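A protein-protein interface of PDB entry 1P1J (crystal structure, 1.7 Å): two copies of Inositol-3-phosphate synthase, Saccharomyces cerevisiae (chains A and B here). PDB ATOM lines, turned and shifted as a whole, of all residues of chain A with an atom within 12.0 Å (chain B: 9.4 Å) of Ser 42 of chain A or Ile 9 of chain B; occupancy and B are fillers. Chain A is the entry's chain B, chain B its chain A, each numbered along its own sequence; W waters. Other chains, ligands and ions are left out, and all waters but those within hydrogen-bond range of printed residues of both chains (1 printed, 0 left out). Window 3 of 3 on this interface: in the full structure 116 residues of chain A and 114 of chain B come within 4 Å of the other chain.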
ATOM      1  N   THR A  38     -13.954  -1.994   5.919  1.00  0.00           N
ATOM      2  CA  THR A  38     -14.019  -0.545   6.069  1.00  0.00           C
ATOM      3  C   THR A  38     -14.535  -0.275   7.477  1.00  0.00           C
ATOM      4  O   THR A  38     -15.399  -0.998   7.972  1.00  0.00           O
ATOM      5  CB  THR A  38     -14.990   0.095   5.060  1.00  0.00           C
ATOM      6  OG1 THR A  38     -16.313  -0.408   5.286  1.00  0.00           O
ATOM      7  CG2 THR A  38     -14.566  -0.221   3.637  1.00  0.00           C
ATOM      8  N   LYS A  39     -14.001   0.751   8.128  1.00  0.00           N
ATOM      9  CA  LYS A  39     -14.438   1.081   9.480  1.00  0.00           C
ATOM     10  C   LYS A  39     -15.108   2.446   9.519  1.00  0.00           C
ATOM     11  O   LYS A  39     -14.581   3.419   8.980  1.00  0.00           O
ATOM     12  CB  LYS A  39     -13.251   1.065  10.445  1.00  0.00           C
ATOM     13  CG  LYS A  39     -13.646   1.292  11.895  1.00  0.00           C
ATOM     14  CD  LYS A  39     -12.436   1.317  12.814  1.00  0.00           C
ATOM     15  CE  LYS A  39     -12.856   1.550  14.256  1.00  0.00           C
ATOM     16  NZ  LYS A  39     -11.687   1.603  15.180  1.00  0.00           N
ATOM     17  N   THR A  40     -16.272   2.513  10.157  1.00  0.00           N
ATOM     18  CA  THR A  40     -17.013   3.764  10.266  1.00  0.00           C
ATOM     19  C   THR A  40     -16.577   4.538  11.504  1.00  0.00           C
ATOM     20  O   THR A  40     -15.939   3.984  12.403  1.00  0.00           O
ATOM     21  CB  THR A  40     -18.525   3.512  10.368  1.00  0.00           C
ATOM     22  OG1 THR A  40     -18.816   2.858  11.609  1.00  0.00           O
ATOM     23  CG2 THR A  40     -18.996   2.636   9.218  1.00  0.00           C
ATOM     24  N   ALA A  41     -16.925   5.820  11.548  1.00  0.00           N
ATOM     25  CA  ALA A  41     -16.573   6.666  12.681  1.00  0.00           C
ATOM     26  C   ALA A  41     -17.186   6.104  13.959  1.00  0.00           C
ATOM     27  O   ALA A  41     -16.596   6.199  15.035  1.00  0.00           O
ATOM     28  CB  ALA A  41     -17.066   8.089  12.443  1.00  0.00           C
ATOM     29  N   SER A  42     -18.371   5.515  13.829  1.00  0.00           N
ATOM     30  CA  SER A  42     -19.068   4.934  14.970  1.00  0.00           C
ATOM     31  C   SER A  42     -18.348   3.691  15.489  1.00  0.00           C
ATOM     32  O   SER A  42     -18.743   3.113  16.503  1.00  0.00           O
ATOM     33  CB  SER A  42     -20.509   4.582  14.584  1.00  0.00           C
ATOM     34  OG  SER A  42     -20.546   3.730  13.452  1.00  0.00           O
ATOM     35  N   GLY A  43     -17.293   3.283  14.787  1.00  0.00           N
ATOM     36  CA  GLY A  43     -16.525   2.124  15.205  1.00  0.00           C
ATOM     37  C   GLY A  43     -17.037   0.787  14.702  1.00  0.00           C
ATOM     38  O   GLY A  43     -16.740  -0.257  15.289  1.00  0.00           O
ATOM     39  N   ARG A  44     -17.805   0.807  13.619  1.00  0.00           N
ATOM     40  CA  ARG A  44     -18.337  -0.431  13.060  1.00  0.00           C
ATOM     41  C   ARG A  44     -17.492  -0.913  11.889  1.00  0.00           C
ATOM     42  O   ARG A  44     -17.176  -0.146  10.978  1.00  0.00           O
ATOM     43  CB  ARG A  44     -19.780  -0.238  12.591  1.00  0.00           C
ATOM     44  CG  ARG A  44     -20.413  -1.508  12.033  1.00  0.00           C
ATOM     45  CD  ARG A  44     -21.744  -1.214  11.365  1.00  0.00           C
ATOM     46  NE  ARG A  44     -21.586  -0.252  10.279  1.00  0.00           N
ATOM     47  CZ  ARG A  44     -22.589   0.233   9.555  1.00  0.00           C
ATOM     48  NH1 ARG A  44     -22.347   1.106   8.587  1.00  0.00           N
ATOM     49  NH2 ARG A  44     -23.834  -0.156   9.799  1.00  0.00           N
ATOM     50  N   PHE A  45     -17.125  -2.188  11.922  1.00  0.00           N
ATOM     51  CA  PHE A  45     -16.331  -2.784  10.857  1.00  0.00           C
ATOM     52  C   PHE A  45     -17.266  -3.474   9.870  1.00  0.00           C
ATOM     53  O   PHE A  45     -17.947  -4.435  10.225  1.00  0.00           O
ATOM     54  CB  PHE A  45     -15.359  -3.819  11.433  1.00  0.00           C
ATOM     55  CG  PHE A  45     -14.230  -3.223  12.228  1.00  0.00           C
ATOM     56  CD1 PHE A  45     -13.082  -2.759  11.593  1.00  0.00           C
ATOM     57  CD2 PHE A  45     -14.310  -3.138  13.615  1.00  0.00           C
ATOM     58  CE1 PHE A  45     -12.026  -2.220  12.329  1.00  0.00           C
ATOM     59  CE2 PHE A  45     -13.261  -2.601  14.359  1.00  0.00           C
ATOM     60  CZ  PHE A  45     -12.119  -2.142  13.717  1.00  0.00           C
ATOM     61  N   ASP A  46     -17.305  -2.975   8.639  1.00  0.00           N
ATOM     62  CA  ASP A  46     -18.143  -3.574   7.608  1.00  0.00           C
ATOM     63  C   ASP A  46     -17.259  -4.491   6.779  1.00  0.00           C
ATOM     64  O   ASP A  46     -16.329  -4.043   6.109  1.00  0.00           O
ATOM     65  CB  ASP A  46     -18.777  -2.491   6.733  1.00  0.00           C
ATOM     66  CG  ASP A  46     -19.833  -1.694   7.475  1.00  0.00           C
ATOM     67  OD1 ASP A  46     -20.792  -2.308   7.988  1.00  0.00           O
ATOM     68  OD2 ASP A  46     -19.707  -0.455   7.547  1.00  0.00           O
ATOM     69  N   VAL A  47     -17.554  -5.784   6.838  1.00  0.00           N
ATOM     70  CA  VAL A  47     -16.767  -6.788   6.136  1.00  0.00           C
ATOM     71  C   VAL A  47     -17.485  -7.362   4.921  1.00  0.00           C
ATOM     72  O   VAL A  47     -18.589  -7.898   5.035  1.00  0.00           O
ATOM     73  CB  VAL A  47     -16.404  -7.940   7.096  1.00  0.00           C
ATOM     74  CG1 VAL A  47     -15.507  -8.946   6.403  1.00  0.00           C
ATOM     75  CG2 VAL A  47     -15.728  -7.376   8.342  1.00  0.00           C
ATOM     76  N   ASP A 385      -4.669  -1.635  18.426  1.00  0.00           N
ATOM     77  CA  ASP A 385      -4.869  -0.281  18.922  1.00  0.00           C
ATOM     78  C   ASP A 385      -5.536  -0.229  20.289  1.00  0.00           C
ATOM     79  O   ASP A 385      -5.893   0.842  20.771  1.00  0.00           O
ATOM     80  CB  ASP A 385      -5.640   0.574  17.903  1.00  0.00           C
ATOM     81  CG  ASP A 385      -7.046   0.072  17.645  1.00  0.00           C
ATOM     82  OD1 ASP A 385      -7.703   0.634  16.744  1.00  0.00           O
ATOM     83  OD2 ASP A 385      -7.498  -0.866  18.331  1.00  0.00           O
ATOM     84  N   ILE A 386      -5.710  -1.390  20.909  1.00  0.00           N
ATOM     85  CA  ILE A 386      -6.270  -1.443  22.256  1.00  0.00           C
ATOM     86  C   ILE A 386      -5.078  -1.133  23.161  1.00  0.00           C
ATOM     87  O   ILE A 386      -5.181  -0.359  24.112  1.00  0.00           O
ATOM     88  CB  ILE A 386      -6.776  -2.853  22.625  1.00  0.00           C
ATOM     89  CG1 ILE A 386      -7.962  -3.241  21.741  1.00  0.00           C
ATOM     90  CG2 ILE A 386      -7.180  -2.888  24.102  1.00  0.00           C
ATOM     91  CD1 ILE A 386      -8.409  -4.691  21.927  1.00  0.00           C
ATOM     92  N   ILE B   9     -18.685   1.860  21.511  1.00  0.00           N
ATOM     93  CA  ILE B   9     -18.829   0.392  21.300  1.00  0.00           C
ATOM     94  C   ILE B   9     -18.469   0.005  19.869  1.00  0.00           C
ATOM     95  O   ILE B   9     -19.053   0.514  18.912  1.00  0.00           O
ATOM     96  CB  ILE B   9     -20.277  -0.073  21.585  1.00  0.00           C
ATOM     97  CG1 ILE B   9     -20.635   0.196  23.048  1.00  0.00           C
ATOM     98  CG2 ILE B   9     -20.424  -1.555  21.265  1.00  0.00           C
ATOM     99  CD1 ILE B   9     -19.771  -0.553  24.048  1.00  0.00           C
ATOM    100  N   THR B  10     -17.504  -0.898  19.730  1.00  0.00           N
ATOM    101  CA  THR B  10     -17.071  -1.359  18.418  1.00  0.00           C
ATOM    102  C   THR B  10     -17.841  -2.619  18.035  1.00  0.00           C
ATOM    103  O   THR B  10     -18.110  -3.474  18.881  1.00  0.00           O
ATOM    104  CB  THR B  10     -15.561  -1.672  18.405  1.00  0.00           C
ATOM    105  OG1 THR B  10     -15.283  -2.731  19.328  1.00  0.00           O
ATOM    106  CG2 THR B  10     -14.762  -0.441  18.803  1.00  0.00           C
ATOM    107  N   SER B  11     -18.200  -2.731  16.762  1.00  0.00           N
ATOM    108  CA  SER B  11     -18.944  -3.890  16.293  1.00  0.00           C
ATOM    109  C   SER B  11     -18.498  -4.319  14.904  1.00  0.00           C
ATOM    110  O   SER B  11     -17.792  -3.589  14.211  1.00  0.00           O
ATOM    111  CB  SER B  11     -20.447  -3.592  16.289  1.00  0.00           C
ATOM    112  OG  SER B  11     -20.748  -2.474  15.471  1.00  0.00           O
ATOM    113  N   VAL B  12     -18.914  -5.514  14.509  1.00  0.00           N
ATOM    114  CA  VAL B  12     -18.558  -6.060  13.210  1.00  0.00           C
ATOM    115  C   VAL B  12     -19.812  -6.545  12.488  1.00  0.00           C
ATOM    116  O   VAL B  12     -20.684  -7.169  13.093  1.00  0.00           O
ATOM    117  CB  VAL B  12     -17.574  -7.244  13.371  1.00  0.00           C
ATOM    118  CG1 VAL B  12     -17.209  -7.812  12.014  1.00  0.00           C
ATOM    119  CG2 VAL B  12     -16.323  -6.785  14.117  1.00  0.00           C
ATOM    120  N   LYS B  62     -26.833 -12.019  25.944  1.00  0.00           N
ATOM    121  CA  LYS B  62     -25.903 -12.399  26.994  1.00  0.00           C
ATOM    122  C   LYS B  62     -26.416 -11.906  28.343  1.00  0.00           C
ATOM    123  O   LYS B  62     -27.132 -10.904  28.423  1.00  0.00           O
ATOM    124  CB  LYS B  62     -24.518 -11.820  26.709  1.00  0.00           C
ATOM    125  CG  LYS B  62     -24.489 -10.314  26.587  1.00  0.00           C
ATOM    126  CD  LYS B  62     -23.111  -9.827  26.172  1.00  0.00           C
ATOM    127  CE  LYS B  62     -23.089  -8.317  26.032  1.00  0.00           C
ATOM    128  NZ  LYS B  62     -21.749  -7.827  25.620  1.00  0.00           N
ATOM    129  N   PRO B 129     -11.000  -5.802  17.760  1.00  0.00           N
ATOM    130  CA  PRO B 129     -10.854  -6.458  19.063  1.00  0.00           C
ATOM    131  C   PRO B 129     -11.412  -7.884  19.044  1.00  0.00           C
ATOM    132  O   PRO B 129     -12.452  -8.147  18.437  1.00  0.00           O
ATOM    133  CB  PRO B 129     -11.648  -5.552  20.000  1.00  0.00           C
ATOM    134  CG  PRO B 129     -11.501  -4.196  19.374  1.00  0.00           C
ATOM    135  CD  PRO B 129     -11.670  -4.495  17.897  1.00  0.00           C
ATOM    136  N   ASN B 131     -12.950  -9.461  21.237  1.00  0.00           N
ATOM    137  CA  ASN B 131     -14.297  -9.522  21.785  1.00  0.00           C
ATOM    138  C   ASN B 131     -15.324  -8.639  21.085  1.00  0.00           C
ATOM    139  O   ASN B 131     -16.382  -8.357  21.646  1.00  0.00           O
ATOM    140  CB  ASN B 131     -14.255  -9.199  23.286  1.00  0.00           C
ATOM    141  CG  ASN B 131     -13.912  -7.748  23.570  1.00  0.00           C
ATOM    142  OD1 ASN B 131     -13.519  -6.998  22.676  1.00  0.00           O
ATOM    143  ND2 ASN B 131     -14.056  -7.347  24.829  1.00  0.00           N
ATOM    144  N   SER B 132     -15.030  -8.224  19.855  1.00  0.00           N
ATOM    145  CA  SER B 132     -15.953  -7.363  19.116  1.00  0.00           C
ATOM    146  C   SER B 132     -16.690  -8.069  17.975  1.00  0.00           C
ATOM    147  O   SER B 132     -17.644  -7.522  17.419  1.00  0.00           O
ATOM    148  CB  SER B 132     -15.210  -6.149  18.549  1.00  0.00           C
ATOM    149  OG  SER B 132     -14.364  -6.527  17.474  1.00  0.00           O
ATOM    150  N   PRO B 135     -21.084 -10.904  20.591  1.00  0.00           N
ATOM    151  CA  PRO B 135     -21.329 -10.506  21.980  1.00  0.00           C
ATOM    152  C   PRO B 135     -20.755 -11.438  23.040  1.00  0.00           C
ATOM    153  O   PRO B 135     -21.071 -12.629  23.077  1.00  0.00           O
ATOM    154  CB  PRO B 135     -22.854 -10.420  22.048  1.00  0.00           C
ATOM    155  CG  PRO B 135     -23.285 -11.469  21.071  1.00  0.00           C
ATOM    156  CD  PRO B 135     -22.353 -11.218  19.909  1.00  0.00           C
ATOM    157  N   MET B 136     -19.905 -10.877  23.896  1.00  0.00           N
ATOM    158  CA  MET B 136     -19.289 -11.618  24.992  1.00  0.00           C
ATOM    159  C   MET B 136     -19.507 -10.820  26.267  1.00  0.00           C
ATOM    160  O   MET B 136     -19.625  -9.595  26.229  1.00  0.00           O
ATOM    161  CB  MET B 136     -17.786 -11.790  24.761  1.00  0.00           C
ATOM    162  CG  MET B 136     -17.436 -12.647  23.560  1.00  0.00           C
ATOM    163  SD  MET B 136     -15.657 -12.742  23.272  1.00  0.00           S
ATOM    164  CE  MET B 136     -15.566 -14.197  22.211  1.00  0.00           C
ATOM    165  N   SER B 138     -18.596  -8.946  29.666  1.00  0.00           N
ATOM    166  CA  SER B 138     -17.434  -8.177  30.096  1.00  0.00           C
ATOM    167  C   SER B 138     -17.078  -8.537  31.532  1.00  0.00           C
ATOM    168  O   SER B 138     -17.961  -8.797  32.347  1.00  0.00           O
ATOM    169  CB  SER B 138     -17.736  -6.680  30.016  1.00  0.00           C
ATOM    170  OG  SER B 138     -16.760  -5.929  30.720  1.00  0.00           O
HETATM  171  O   HOH W   1     -20.569   0.129  16.566  1.00  0.00           O
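The backbone NH (N) of Ser 11 of chain B is in hydrogen-bond range of the backbone carbonyl oxygen (O) of Gly 43 of chain A (3.2 Å). N of Phe 45 of chain A is in hydrogen-bond range of O of Ser 11 of chain B (2.8 Å).
OG1 of Thr 40 of chain A is in hydrogen-bond range of N of Arg 44 of chain A, 3.0 Å away. The side-chain hydroxyl (OG) of Ser 132 of chain B is in hydrogen-bond range of the backbone carbonyl oxygen (O) of Pro 129 of chain B, 2.7 Å away. The side-chain hydroxyl (OG1) of Thr 40 of chain A sits at hydrogen-bond distance from the side-chain hydroxyl (OG) of Ser 42 of chain A (2.7 Å). NE of Arg 44 of chain A lies within salt-bridge range of OD1 of Asp 46 of chain A.
Ser 42 of chain A touches Ile 9 of chain B. O of Gly 43 of chain A touches CA of Thr 10 of chain B, at 3.3 Å. CA of Arg 44 of chain A touches O of Ser 11 of chain B (3.4 Å). Val 12 of chain B touches Phe 45 of chain A. Val 47 of chain A touches Val 12 of chain B (CG2 to CG1, 3.98 Å). CD1 of Ile 386 of chain A touches CB of Pro 129 of chain B (3.9 Å).
Of chain B, only Ile 9 (3.6 Å) comes within 4 Å of Ser 42 of chain A. Of chain A, only Ser 42 (3.6 Å) comes within 4 Å of Ile 9 of chain B. No residue of chain B comes within 4 Å of Thr 40 of chain A. No residue of chain B comes within 4 Å of Ala 41 of chain A. Printed residues of chain B within 4 Å of Gly 43 of chain A: Thr 10 (3.3 Å) and Ser 11 (3.2 Å). Thr 10 of chain B touches one residue of chain A. Printed residues of chain A within 4 Å of Pro 129 of chain B: Ile 386. Of the printed residues of chain B, Val 47 of chain A touches Val 12 (3.98 Å). Of the printed residues of chain B, Arg 44 of chain A touches Ser 11 (3.4 Å). Of the printed residues of chain B, Phe 45 of chain A touches Ser 11 and Val 12. Printed residues of chain A within 4 Å of Val 12 of chain B: Phe 45 and Val 47. The nearest residue of chain B that does not touch Ser 42 of chain A is Thr 10 of chain B (5.1 Å). The nearest printed residue of chain B that does not touch Phe 45 of chain A is Pro 129 of chain B (4.3 Å).
Hydrophobic or aromatic side chains of chain B that line the printed part of chain A: Val 12 and Pro 129. Printed residues of chain A that touch a printed residue of chain B: Ser 42, Gly 43, Arg 44, Phe 45, Val 47 and Ile 386. Hydrophobic or aromatic side chains of chain A that line the printed part of chain B: Phe 45, Val 47 and Ile 386. Among the printed residues, no Asp or Glu carboxylate lies within 4 Å of a Lys or Arg side-chain nitrogen of the other chain.
No position is printed for both chains.
Water W1 lies within hydrogen-bond range of the backbone carbonyl oxygen (O) of Ile 9 of chain B (2.8 Å), the side-chain hydroxyl (OG) of Ser 11 of chain B (2.8 Å) and the backbone carbonyl oxygen (O) of Ser 42 of chain A (3.5 Å).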
